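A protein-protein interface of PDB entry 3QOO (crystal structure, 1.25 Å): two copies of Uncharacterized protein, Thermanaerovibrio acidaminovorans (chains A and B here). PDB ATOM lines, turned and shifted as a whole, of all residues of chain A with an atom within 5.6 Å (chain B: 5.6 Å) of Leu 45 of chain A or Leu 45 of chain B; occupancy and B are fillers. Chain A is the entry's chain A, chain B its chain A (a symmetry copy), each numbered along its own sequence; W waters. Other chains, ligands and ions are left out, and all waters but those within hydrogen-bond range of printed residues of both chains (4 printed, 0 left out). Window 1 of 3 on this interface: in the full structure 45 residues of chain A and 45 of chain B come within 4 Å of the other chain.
The backbone NH of Ala 42 of chain A lies close to the side-chain hydroxyl of Ser 40 of chain A (3.4 Å). OG1 of Thr 49 of chain A is in hydrogen-bond range of O of Leu 45 of chain A. The side-chain amide nitrogen (NE2) of Gln 117 of chain A lies within hydrogen-bond range of the side-chain hydroxyl (OG) of Ser 71 of chain A, at 2.9 Å. The side-chain hydroxyl (OG) of Ser 40 of chain B sits close to the backbone NH (N) of Ala 42 of chain B, at 3.4 Å. O of Leu 45 of chain B lies within hydrogen-bond range of OG1 of Thr 49 of chain B (3.1 Å). OG of Ser 71 of chain B is in hydrogen-bond range of NE2 of Gln 117 of chain B, at 2.9 Å.
The backbone carbonyl oxygen (O) of Ser 71 of chain A lies within hydrogen-bond range of the backbone NH (N) of Val 73 of chain B (2.9 Å). The backbone NH (N) of Val 73 of chain A is in hydrogen-bond range of the backbone carbonyl oxygen (O) of Ser 71 of chain B, 2.9 Å away.
Among the printed residues, merely in contact across the chains: Thr 41 of chain A with Leu 45 of chain B (3.9 Å), Thr 41 of chain A with Ser 71 of chain B (3.9 Å), Ala 42 of chain A with Ala 42 of chain B (3.9 Å), Leu 45 of chain A with Thr 41 of chain B (3.9 Å), Leu 45 of chain A with Leu 45 of chain B (2.8 Å) and Ser 71 of chain A with Thr 41 of chain B (3.9 Å).
Water W4 lies within hydrogen-bond range of OG1 of Thr 49 of chain A, NE2 of Gln 117 of chain A and OG1 of Thr 41 of chain B. Water W3 lies within hydrogen-bond range of the side-chain hydroxyl of Thr 49 of chain B (3.1 Å), the side-chain amide nitrogen of Gln 117 of chain B (3.4 Å) and the side-chain hydroxyl of Thr 41 of chain A (3.4 Å). Water W1 lies within hydrogen-bond range of the side-chain hydroxyl (OG1) of Thr 49 of chain A (3.2 Å) and the backbone NH (N) of Ala 42 of chain B (3.2 Å). Water W2 bridges OG1 of Thr 49 of chain B (3.2 Å) and N of Ala 42 of chain A (3.2 Å).
Leu 45 of chain A touches just these residues of chain B: Thr 41 (3.9 Å) and Leu 45 (2.8 Å). Leu 45 of chain B touches two residues of chain A. Of the printed residues of chain B, Val 73 of chain A touches Ser 71 (2.9 Å). Printed residues of chain B within 4 Å of Thr 41 of chain A: Leu 45 (3.9 Å) and Ser 71 (3.9 Å). The nearest printed residue of chain A that does not touch Val 73 of chain B is Leu 45 of chain A (5.1 Å).
Thr 41 of chain A touches Leu 45 of chain B, and with the chains exchanged Leu 45 of chain A touches Thr 41 of chain B. Thr 41 of chain A touches Ser 71 of chain B, and with the chains exchanged Ser 71 of chain A touches Thr 41 of chain B. Ala 42 of chain B touches its own counterpart, Ala 42 of chain A. Leu 45 of chain A touches its own counterpart, Leu 45 of chain B. 15 positions are printed for both chains. Of the 8 pairs that touch across the chains among the printed residues, 8 have their exchanged pair printed and touching as well.
Of the 15 printed residues of chain B, 5 touch a printed residue of chain A. Printed residues of chain B that touch a printed residue of chain A: Thr 41, Ala 42, Leu 45, Ser 71 and Val 73. Hydrophobic or aromatic side chains of chain B that line the printed part of chain A: Ala 42 and Leu 45. Printed residues of chain A that touch a printed residue of chain B: Thr 41, Ala 42, Leu 45, Ser 71 and Val 73. Hydrophobic or aromatic side chains of chain A within 4 Å of the printed part of chain B: Ala 42 and Leu 45. Among the printed residues, 8 pairs touch across the chains.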
ATOM      1  N   SER A  40      -2.160   4.867  30.221  1.00  0.00           N
ATOM      2  CA  SER A  40      -2.685   3.598  30.743  1.00  0.00           C
ATOM      3  C   SER A  40      -2.046   2.391  30.073  1.00  0.00           C
ATOM      4  O   SER A  40      -1.486   2.446  28.966  1.00  0.00           O
ATOM      5  CB  SER A  40      -4.169   3.527  30.485  1.00  0.00           C
ATOM      6  OG  SER A  40      -4.420   3.310  29.116  1.00  0.00           O
ATOM      7  N   THR A  41      -2.171   1.252  30.726  1.00  0.00           N
ATOM      8  CA  THR A  41      -1.706   0.009  30.145  1.00  0.00           C
ATOM      9  C   THR A  41      -2.419  -0.298  28.837  1.00  0.00           C
ATOM     10  O   THR A  41      -1.788  -0.752  27.888  1.00  0.00           O
ATOM     11  CB  THR A  41      -1.889  -1.144  31.110  1.00  0.00           C
ATOM     12  OG1 THR A  41      -1.318  -0.767  32.373  1.00  0.00           O
ATOM     13  CG2 THR A  41      -1.182  -2.407  30.606  1.00  0.00           C
ATOM     14  N   ALA A  42      -3.715  -0.026  28.769  1.00  0.00           N
ATOM     15  CA  ALA A  42      -4.475  -0.258  27.549  1.00  0.00           C
ATOM     16  C   ALA A  42      -3.913   0.566  26.398  1.00  0.00           C
ATOM     17  O   ALA A  42      -3.842   0.087  25.248  1.00  0.00           O
ATOM     18  CB  ALA A  42      -5.958   0.081  27.735  1.00  0.00           C
ATOM     19  N   ALA A  43      -3.494   1.798  26.674  1.00  0.00           N
ATOM     20  CA  ALA A  43      -2.903   2.647  25.647  1.00  0.00           C
ATOM     21  C   ALA A  43      -1.580   2.086  25.166  1.00  0.00           C
ATOM     22  O   ALA A  43      -1.294   2.120  23.964  1.00  0.00           O
ATOM     23  CB  ALA A  43      -2.721   4.063  26.166  1.00  0.00           C
ATOM     24  N   PHE A  44      -0.728   1.640  26.068  1.00  0.00           N
ATOM     25  CA  PHE A  44       0.513   0.977  25.653  1.00  0.00           C
ATOM     26  C   PHE A  44       0.216  -0.204  24.763  1.00  0.00           C
ATOM     27  O   PHE A  44       0.876  -0.407  23.734  1.00  0.00           O
ATOM     28  CB  PHE A  44       1.346   0.529  26.851  1.00  0.00           C
ATOM     29  CG  PHE A  44       2.047   1.645  27.556  1.00  0.00           C
ATOM     30  CD1 PHE A  44       3.151   2.245  27.016  1.00  0.00           C
ATOM     31  CD2 PHE A  44       1.659   2.045  28.811  1.00  0.00           C
ATOM     32  CE1 PHE A  44       3.805   3.258  27.647  1.00  0.00           C
ATOM     33  CE2 PHE A  44       2.332   3.057  29.471  1.00  0.00           C
ATOM     34  CZ  PHE A  44       3.402   3.665  28.890  1.00  0.00           C
ATOM     35  N   LEU A  45      -0.797  -0.988  25.129  1.00  0.00           N
ATOM     36  CA  LEU A  45      -1.171  -2.160  24.354  1.00  0.00           C
ATOM     37  C   LEU A  45      -1.694  -1.771  22.963  1.00  0.00           C
ATOM     38  O   LEU A  45      -1.282  -2.351  21.953  1.00  0.00           O
ATOM     39  CB  LEU A  45      -2.185  -2.993  25.131  1.00  0.00           C
ATOM     40  CG  LEU A  45      -2.215  -4.494  24.856  1.00  0.00           C
ATOM     41  CD1 LEU A  45      -2.962  -5.204  25.953  1.00  0.00           C
ATOM     42  CD2 LEU A  45      -2.804  -4.833  23.511  1.00  0.00           C
ATOM     43  N   GLU A  46      -2.591  -0.801  22.897  1.00  0.00           N
ATOM     44  CA  GLU A  46      -3.146  -0.372  21.627  1.00  0.00           C
ATOM     45  C   GLU A  46      -2.022   0.049  20.661  1.00  0.00           C
ATOM     46  O   GLU A  46      -2.057  -0.238  19.462  1.00  0.00           O
ATOM     47  CB  GLU A  46      -4.107   0.793  21.853  1.00  0.00           C
ATOM     48  CG  GLU A  46      -4.726   1.298  20.587  1.00  0.00           C
ATOM     49  CD  GLU A  46      -5.596   2.513  20.792  1.00  0.00           C
ATOM     50  OE1 GLU A  46      -5.909   2.842  21.957  1.00  0.00           O
ATOM     51  OE2 GLU A  46      -5.968   3.121  19.765  1.00  0.00           O
ATOM     52  N   THR A  47      -1.024   0.761  21.184  1.00  0.00           N
ATOM     53  CA  THR A  47       0.044   1.278  20.352  1.00  0.00           C
ATOM     54  C   THR A  47       0.966   0.145  19.873  1.00  0.00           C
ATOM     55  O   THR A  47       1.399   0.105  18.723  1.00  0.00           O
ATOM     56  CB  THR A  47       0.820   2.365  21.092  1.00  0.00           C
ATOM     57  OG1 THR A  47      -0.087   3.354  21.640  1.00  0.00           O
ATOM     58  CG2 THR A  47       1.824   2.980  20.160  1.00  0.00           C
ATOM     59  N   MET A  48       1.233  -0.804  20.763  1.00  0.00           N
ATOM     60  CA  MET A  48       1.948  -2.000  20.399  1.00  0.00           C
ATOM     61  C   MET A  48       1.243  -2.752  19.272  1.00  0.00           C
ATOM     62  O   MET A  48       1.880  -3.170  18.288  1.00  0.00           O
ATOM     63  CB  MET A  48       2.130  -2.897  21.619  1.00  0.00           C
ATOM     64  CG  MET A  48       2.792  -4.245  21.278  1.00  0.00           C
ATOM     65  SD  MET A  48       3.354  -5.268  22.864  1.00  0.00           S
ATOM     66  CE  MET A  48       1.616  -5.536  23.725  1.00  0.00           C
ATOM     67  N   THR A  49      -0.069  -2.888  19.402  1.00  0.00           N
ATOM     68  CA  THR A  49      -0.890  -3.556  18.395  1.00  0.00           C
ATOM     69  C   THR A  49      -0.765  -2.821  17.047  1.00  0.00           C
ATOM     70  O   THR A  49      -0.580  -3.438  15.997  1.00  0.00           O
ATOM     71  CB  THR A  49      -2.351  -3.642  18.815  1.00  0.00           C
ATOM     72  OG1 THR A  49      -2.424  -4.487  19.961  1.00  0.00           O
ATOM     73  CG2 THR A  49      -3.185  -4.207  17.697  1.00  0.00           C
ATOM     74  N   GLN A  50      -0.896  -1.504  17.081  1.00  0.00           N
ATOM     75  CA  GLN A  50      -0.798  -0.718  15.861  1.00  0.00           C
ATOM     76  C   GLN A  50       0.513  -0.964  15.131  1.00  0.00           C
ATOM     77  O   GLN A  50       0.516  -1.189  13.909  1.00  0.00           O
ATOM     78  CB  GLN A  50      -0.930   0.777  16.171  1.00  0.00           C
ATOM     79  CG  GLN A  50      -0.809   1.625  14.919  1.00  0.00           C
ATOM     80  CD  GLN A  50      -0.932   3.091  15.169  1.00  0.00           C
ATOM     81  OE1 GLN A  50      -1.350   3.499  16.249  1.00  0.00           O
ATOM     82  NE2 GLN A  50      -0.633   3.903  14.154  1.00  0.00           N
ATOM     83  N   SER A  71      -1.124 -10.776  24.581  1.00  0.00           N
ATOM     84  CA  SER A  71      -0.336  -9.573  24.841  1.00  0.00           C
ATOM     85  C   SER A  71       0.053  -9.503  26.290  1.00  0.00           C
ATOM     86  O   SER A  71      -0.716  -9.932  27.171  1.00  0.00           O
ATOM     87  CB  SER A  71      -1.098  -8.316  24.457  1.00  0.00           C
ATOM     88  OG  SER A  71      -1.288  -8.226  23.054  1.00  0.00           O
ATOM     89  N   VAL A  73       2.088  -6.522  28.994  1.00  0.00           N
ATOM     90  CA  VAL A  73       2.723  -5.228  29.190  1.00  0.00           C
ATOM     91  C   VAL A  73       3.250  -5.148  30.602  1.00  0.00           C
ATOM     92  O   VAL A  73       2.547  -5.533  31.552  1.00  0.00           O
ATOM     93  CB  VAL A  73       1.738  -4.052  28.898  1.00  0.00           C
ATOM     94  CG1 VAL A  73       2.383  -2.686  29.206  1.00  0.00           C
ATOM     95  CG2 VAL A  73       1.271  -4.114  27.471  1.00  0.00           C
ATOM     96  N   MET A 103       8.300  -5.326  22.565  1.00  0.00           N
ATOM     97  CA  MET A 103       8.013  -3.897  22.566  1.00  0.00           C
ATOM     98  C   MET A 103       8.789  -3.215  23.668  1.00  0.00           C
ATOM     99  O   MET A 103       8.915  -3.738  24.785  1.00  0.00           O
ATOM    100  CB  MET A 103       6.502  -3.656  22.776  1.00  0.00           C
ATOM    101  CG  MET A 103       6.051  -2.227  22.764  1.00  0.00           C
ATOM    102  SD  MET A 103       6.134  -1.327  24.491  1.00  0.00           S
ATOM    103  CE  MET A 103       4.435  -1.970  25.232  1.00  0.00           C
ATOM    104  N   GLN A 117       3.748  -9.296  22.165  1.00  0.00           N
ATOM    105  CA  GLN A 117       2.500  -9.645  21.515  1.00  0.00           C
ATOM    106  C   GLN A 117       2.723 -10.821  20.577  1.00  0.00           C
ATOM    107  O   GLN A 117       3.680 -10.814  19.785  1.00  0.00           O
ATOM    108  CB  GLN A 117       1.916  -8.458  20.775  1.00  0.00           C
ATOM    109  CG  GLN A 117       0.508  -8.726  20.199  1.00  0.00           C
ATOM    110  CD  GLN A 117      -0.134  -7.460  19.724  1.00  0.00           C
ATOM    111  OE1 GLN A 117      -0.110  -7.151  18.528  1.00  0.00           O
ATOM    112  NE2 GLN A 117      -0.680  -6.680  20.664  1.00  0.00           N
ATOM    113  N   SER B  40     -11.180  -5.826  20.724  1.00  0.00           N
ATOM    114  CA  SER B  40      -9.712  -5.804  20.710  1.00  0.00           C
ATOM    115  C   SER B  40      -9.118  -6.228  22.045  1.00  0.00           C
ATOM    116  O   SER B  40      -9.750  -6.188  23.113  1.00  0.00           O
ATOM    117  CB  SER B  40      -9.235  -4.403  20.426  1.00  0.00           C
ATOM    118  OG  SER B  40      -9.445  -3.575  21.546  1.00  0.00           O
ATOM    119  N   THR B  41      -7.852  -6.597  22.007  1.00  0.00           N
ATOM    120  CA  THR B  41      -7.136  -6.917  23.224  1.00  0.00           C
ATOM    121  C   THR B  41      -7.089  -5.730  24.173  1.00  0.00           C
ATOM    122  O   THR B  41      -7.245  -5.902  25.378  1.00  0.00           O
ATOM    123  CB  THR B  41      -5.727  -7.385  22.920  1.00  0.00           C
ATOM    124  OG1 THR B  41      -5.802  -8.417  21.924  1.00  0.00           O
ATOM    125  CG2 THR B  41      -5.049  -7.954  24.170  1.00  0.00           C
ATOM    126  N   ALA B  42      -6.906  -4.529  23.642  1.00  0.00           N
ATOM    127  CA  ALA B  42      -6.877  -3.330  24.467  1.00  0.00           C
ATOM    128  C   ALA B  42      -8.194  -3.156  25.211  1.00  0.00           C
ATOM    129  O   ALA B  42      -8.210  -2.750  26.391  1.00  0.00           O
ATOM    130  CB  ALA B  42      -6.599  -2.076  23.632  1.00  0.00           C
ATOM    131  N   ALA B  43      -9.312  -3.464  24.559  1.00  0.00           N
ATOM    132  CA  ALA B  43     -10.617  -3.368  25.201  1.00  0.00           C
ATOM    133  C   ALA B  43     -10.752  -4.378  26.322  1.00  0.00           C
ATOM    134  O   ALA B  43     -11.305  -4.059  27.380  1.00  0.00           O
ATOM    135  CB  ALA B  43     -11.728  -3.557  24.181  1.00  0.00           C
ATOM    136  N   PHE B  44     -10.335  -5.610  26.105  1.00  0.00           N
ATOM    137  CA  PHE B  44     -10.330  -6.595  27.190  1.00  0.00           C
ATOM    138  C   PHE B  44      -9.516  -6.098  28.359  1.00  0.00           C
ATOM    139  O   PHE B  44      -9.931  -6.220  29.521  1.00  0.00           O
ATOM    140  CB  PHE B  44      -9.800  -7.950  26.727  1.00  0.00           C
ATOM    141  CG  PHE B  44     -10.761  -8.723  25.882  1.00  0.00           C
ATOM    142  CD1 PHE B  44     -11.852  -9.340  26.429  1.00  0.00           C
ATOM    143  CD2 PHE B  44     -10.531  -8.913  24.542  1.00  0.00           C
ATOM    144  CE1 PHE B  44     -12.733 -10.051  25.676  1.00  0.00           C
ATOM    145  CE2 PHE B  44     -11.408  -9.656  23.772  1.00  0.00           C
ATOM    146  CZ  PHE B  44     -12.509 -10.222  24.337  1.00  0.00           C
ATOM    147  N   LEU B  45      -8.358  -5.506  28.072  1.00  0.00           N
ATOM    148  CA  LEU B  45      -7.485  -4.994  29.116  1.00  0.00           C
ATOM    149  C   LEU B  45      -8.138  -3.827  29.873  1.00  0.00           C
ATOM    150  O   LEU B  45      -8.133  -3.800  31.108  1.00  0.00           O
ATOM    151  CB  LEU B  45      -6.137  -4.601  28.518  1.00  0.00           C
ATOM    152  CG  LEU B  45      -4.919  -4.673  29.434  1.00  0.00           C
ATOM    153  CD1 LEU B  45      -3.657  -4.644  28.615  1.00  0.00           C
ATOM    154  CD2 LEU B  45      -4.899  -3.581  30.472  1.00  0.00           C
ATOM    155  N   GLU B  46      -8.699  -2.869  29.153  1.00  0.00           N
ATOM    156  CA  GLU B  46      -9.333  -1.727  29.782  1.00  0.00           C
ATOM    157  C   GLU B  46     -10.426  -2.188  30.765  1.00  0.00           C
ATOM    158  O   GLU B  46     -10.590  -1.639  31.857  1.00  0.00           O
ATOM    159  CB  GLU B  46      -9.938  -0.821  28.712  1.00  0.00           C
ATOM    160  CG  GLU B  46     -10.615   0.388  29.279  1.00  0.00           C
ATOM    161  CD  GLU B  46     -11.302   1.232  28.236  1.00  0.00           C
ATOM    162  OE1 GLU B  46     -11.068   1.008  27.028  1.00  0.00           O
ATOM    163  OE2 GLU B  46     -12.068   2.129  28.649  1.00  0.00           O
ATOM    164  N   THR B  47     -11.201  -3.194  30.362  1.00  0.00           N
ATOM    165  CA  THR B  47     -12.312  -3.656  31.171  1.00  0.00           C
ATOM    166  C   THR B  47     -11.811  -4.404  32.416  1.00  0.00           C
ATOM    167  O   THR B  47     -12.332  -4.247  33.519  1.00  0.00           O
ATOM    168  CB  THR B  47     -13.260  -4.514  30.337  1.00  0.00           C
ATOM    169  OG1 THR B  47     -13.617  -3.833  29.109  1.00  0.00           O
ATOM    170  CG2 THR B  47     -14.470  -4.857  31.159  1.00  0.00           C
ATOM    171  N   MET B  48     -10.761  -5.197  32.236  1.00  0.00           N
ATOM    172  CA  MET B  48     -10.094  -5.829  33.346  1.00  0.00           C
ATOM    173  C   MET B  48      -9.598  -4.800  34.360  1.00  0.00           C
ATOM    174  O   MET B  48      -9.801  -4.956  35.578  1.00  0.00           O
ATOM    175  CB  MET B  48      -8.942  -6.694  32.844  1.00  0.00           C
ATOM    176  CG  MET B  48      -8.117  -7.314  33.987  1.00  0.00           C
ATOM    177  SD  MET B  48      -6.856  -8.701  33.384  1.00  0.00           S
ATOM    178  CE  MET B  48      -5.723  -7.633  32.196  1.00  0.00           C
ATOM    179  N   THR B  49      -8.984  -3.740  33.854  1.00  0.00           N
ATOM    180  CA  THR B  49      -8.480  -2.654  34.689  1.00  0.00           C
ATOM    181  C   THR B  49      -9.641  -2.019  35.480  1.00  0.00           C
ATOM    182  O   THR B  49      -9.539  -1.781  36.684  1.00  0.00           O
ATOM    183  CB  THR B  49      -7.756  -1.593  33.872  1.00  0.00           C
ATOM    184  OG1 THR B  49      -6.590  -2.194  33.316  1.00  0.00           O
ATOM    185  CG2 THR B  49      -7.376  -0.428  34.746  1.00  0.00           C
ATOM    186  N   GLN B  50     -10.729  -1.723  34.788  1.00  0.00           N
ATOM    187  CA  GLN B  50     -11.880  -1.118  35.441  1.00  0.00           C
ATOM    188  C   GLN B  50     -12.372  -1.953  36.612  1.00  0.00           C
ATOM    189  O   GLN B  50     -12.611  -1.416  37.706  1.00  0.00           O
ATOM    190  CB  GLN B  50     -13.026  -0.923  34.442  1.00  0.00           C
ATOM    191  CG  GLN B  50     -14.249  -0.313  35.100  1.00  0.00           C
ATOM    192  CD  GLN B  50     -15.393  -0.102  34.166  1.00  0.00           C
ATOM    193  OE1 GLN B  50     -15.223  -0.183  32.954  1.00  0.00           O
ATOM    194  NE2 GLN B  50     -16.563   0.237  34.713  1.00  0.00           N
ATOM    195  N   SER B  71       0.077  -6.441  32.990  1.00  0.00           N
ATOM    196  CA  SER B  71      -1.147  -7.067  32.495  1.00  0.00           C
ATOM    197  C   SER B  71      -0.827  -8.074  31.427  1.00  0.00           C
ATOM    198  O   SER B  71       0.122  -7.883  30.644  1.00  0.00           O
ATOM    199  CB  SER B  71      -2.117  -6.033  31.946  1.00  0.00           C
ATOM    200  OG  SER B  71      -2.628  -5.196  32.971  1.00  0.00           O
ATOM    201  N   VAL B  73      -3.158 -10.664  28.564  1.00  0.00           N
ATOM    202  CA  VAL B  73      -4.432 -11.113  28.024  1.00  0.00           C
ATOM    203  C   VAL B  73      -4.181 -12.222  27.031  1.00  0.00           C
ATOM    204  O   VAL B  73      -3.268 -12.114  26.194  1.00  0.00           O
ATOM    205  CB  VAL B  73      -5.221  -9.942  27.359  1.00  0.00           C
ATOM    206  CG1 VAL B  73      -6.521 -10.441  26.698  1.00  0.00           C
ATOM    207  CG2 VAL B  73      -5.514  -8.876  28.377  1.00  0.00           C
ATOM    208  N   MET B 103      -8.603 -12.874  35.406  1.00  0.00           N
ATOM    209  CA  MET B 103      -9.748 -12.409  34.634  1.00  0.00           C
ATOM    210  C   MET B 103     -10.216 -13.499  33.698  1.00  0.00           C
ATOM    211  O   MET B 103      -9.408 -14.211  33.085  1.00  0.00           O
ATOM    212  CB  MET B 103      -9.366 -11.157  33.815  1.00  0.00           C
ATOM    213  CG  MET B 103     -10.460 -10.543  32.994  1.00  0.00           C
ATOM    214  SD  MET B 103     -10.659 -11.289  31.205  1.00  0.00           S
ATOM    215  CE  MET B 103      -9.256 -10.255  30.304  1.00  0.00           C
ATOM    216  N   GLN B 117      -3.733  -9.324  35.978  1.00  0.00           N
ATOM    217  CA  GLN B 117      -3.233  -7.985  36.224  1.00  0.00           C
ATOM    218  C   GLN B 117      -2.619  -7.917  37.614  1.00  0.00           C
ATOM    219  O   GLN B 117      -3.233  -8.378  38.591  1.00  0.00           O
ATOM    220  CB  GLN B 117      -4.329  -6.951  36.059  1.00  0.00           C
ATOM    221  CG  GLN B 117      -3.819  -5.496  36.151  1.00  0.00           C
ATOM    222  CD  GLN B 117      -4.870  -4.524  35.714  1.00  0.00           C
ATOM    223  OE1 GLN B 117      -5.570  -3.937  36.545  1.00  0.00           O
ATOM    224  NE2 GLN B 117      -5.028  -4.372  34.394  1.00  0.00           N
HETATM  225  O   HOH W   1      -5.396  -3.844  20.881  1.00  0.00           O
HETATM  226  O   HOH W   2      -5.806   0.057  31.216  1.00  0.00           O
HETATM  227  O   HOH W   3      -3.897  -1.218  34.603  1.00  0.00           O
HETATM  228  O   HOH W   4      -3.737  -7.287  19.417  1.00  0.00           O
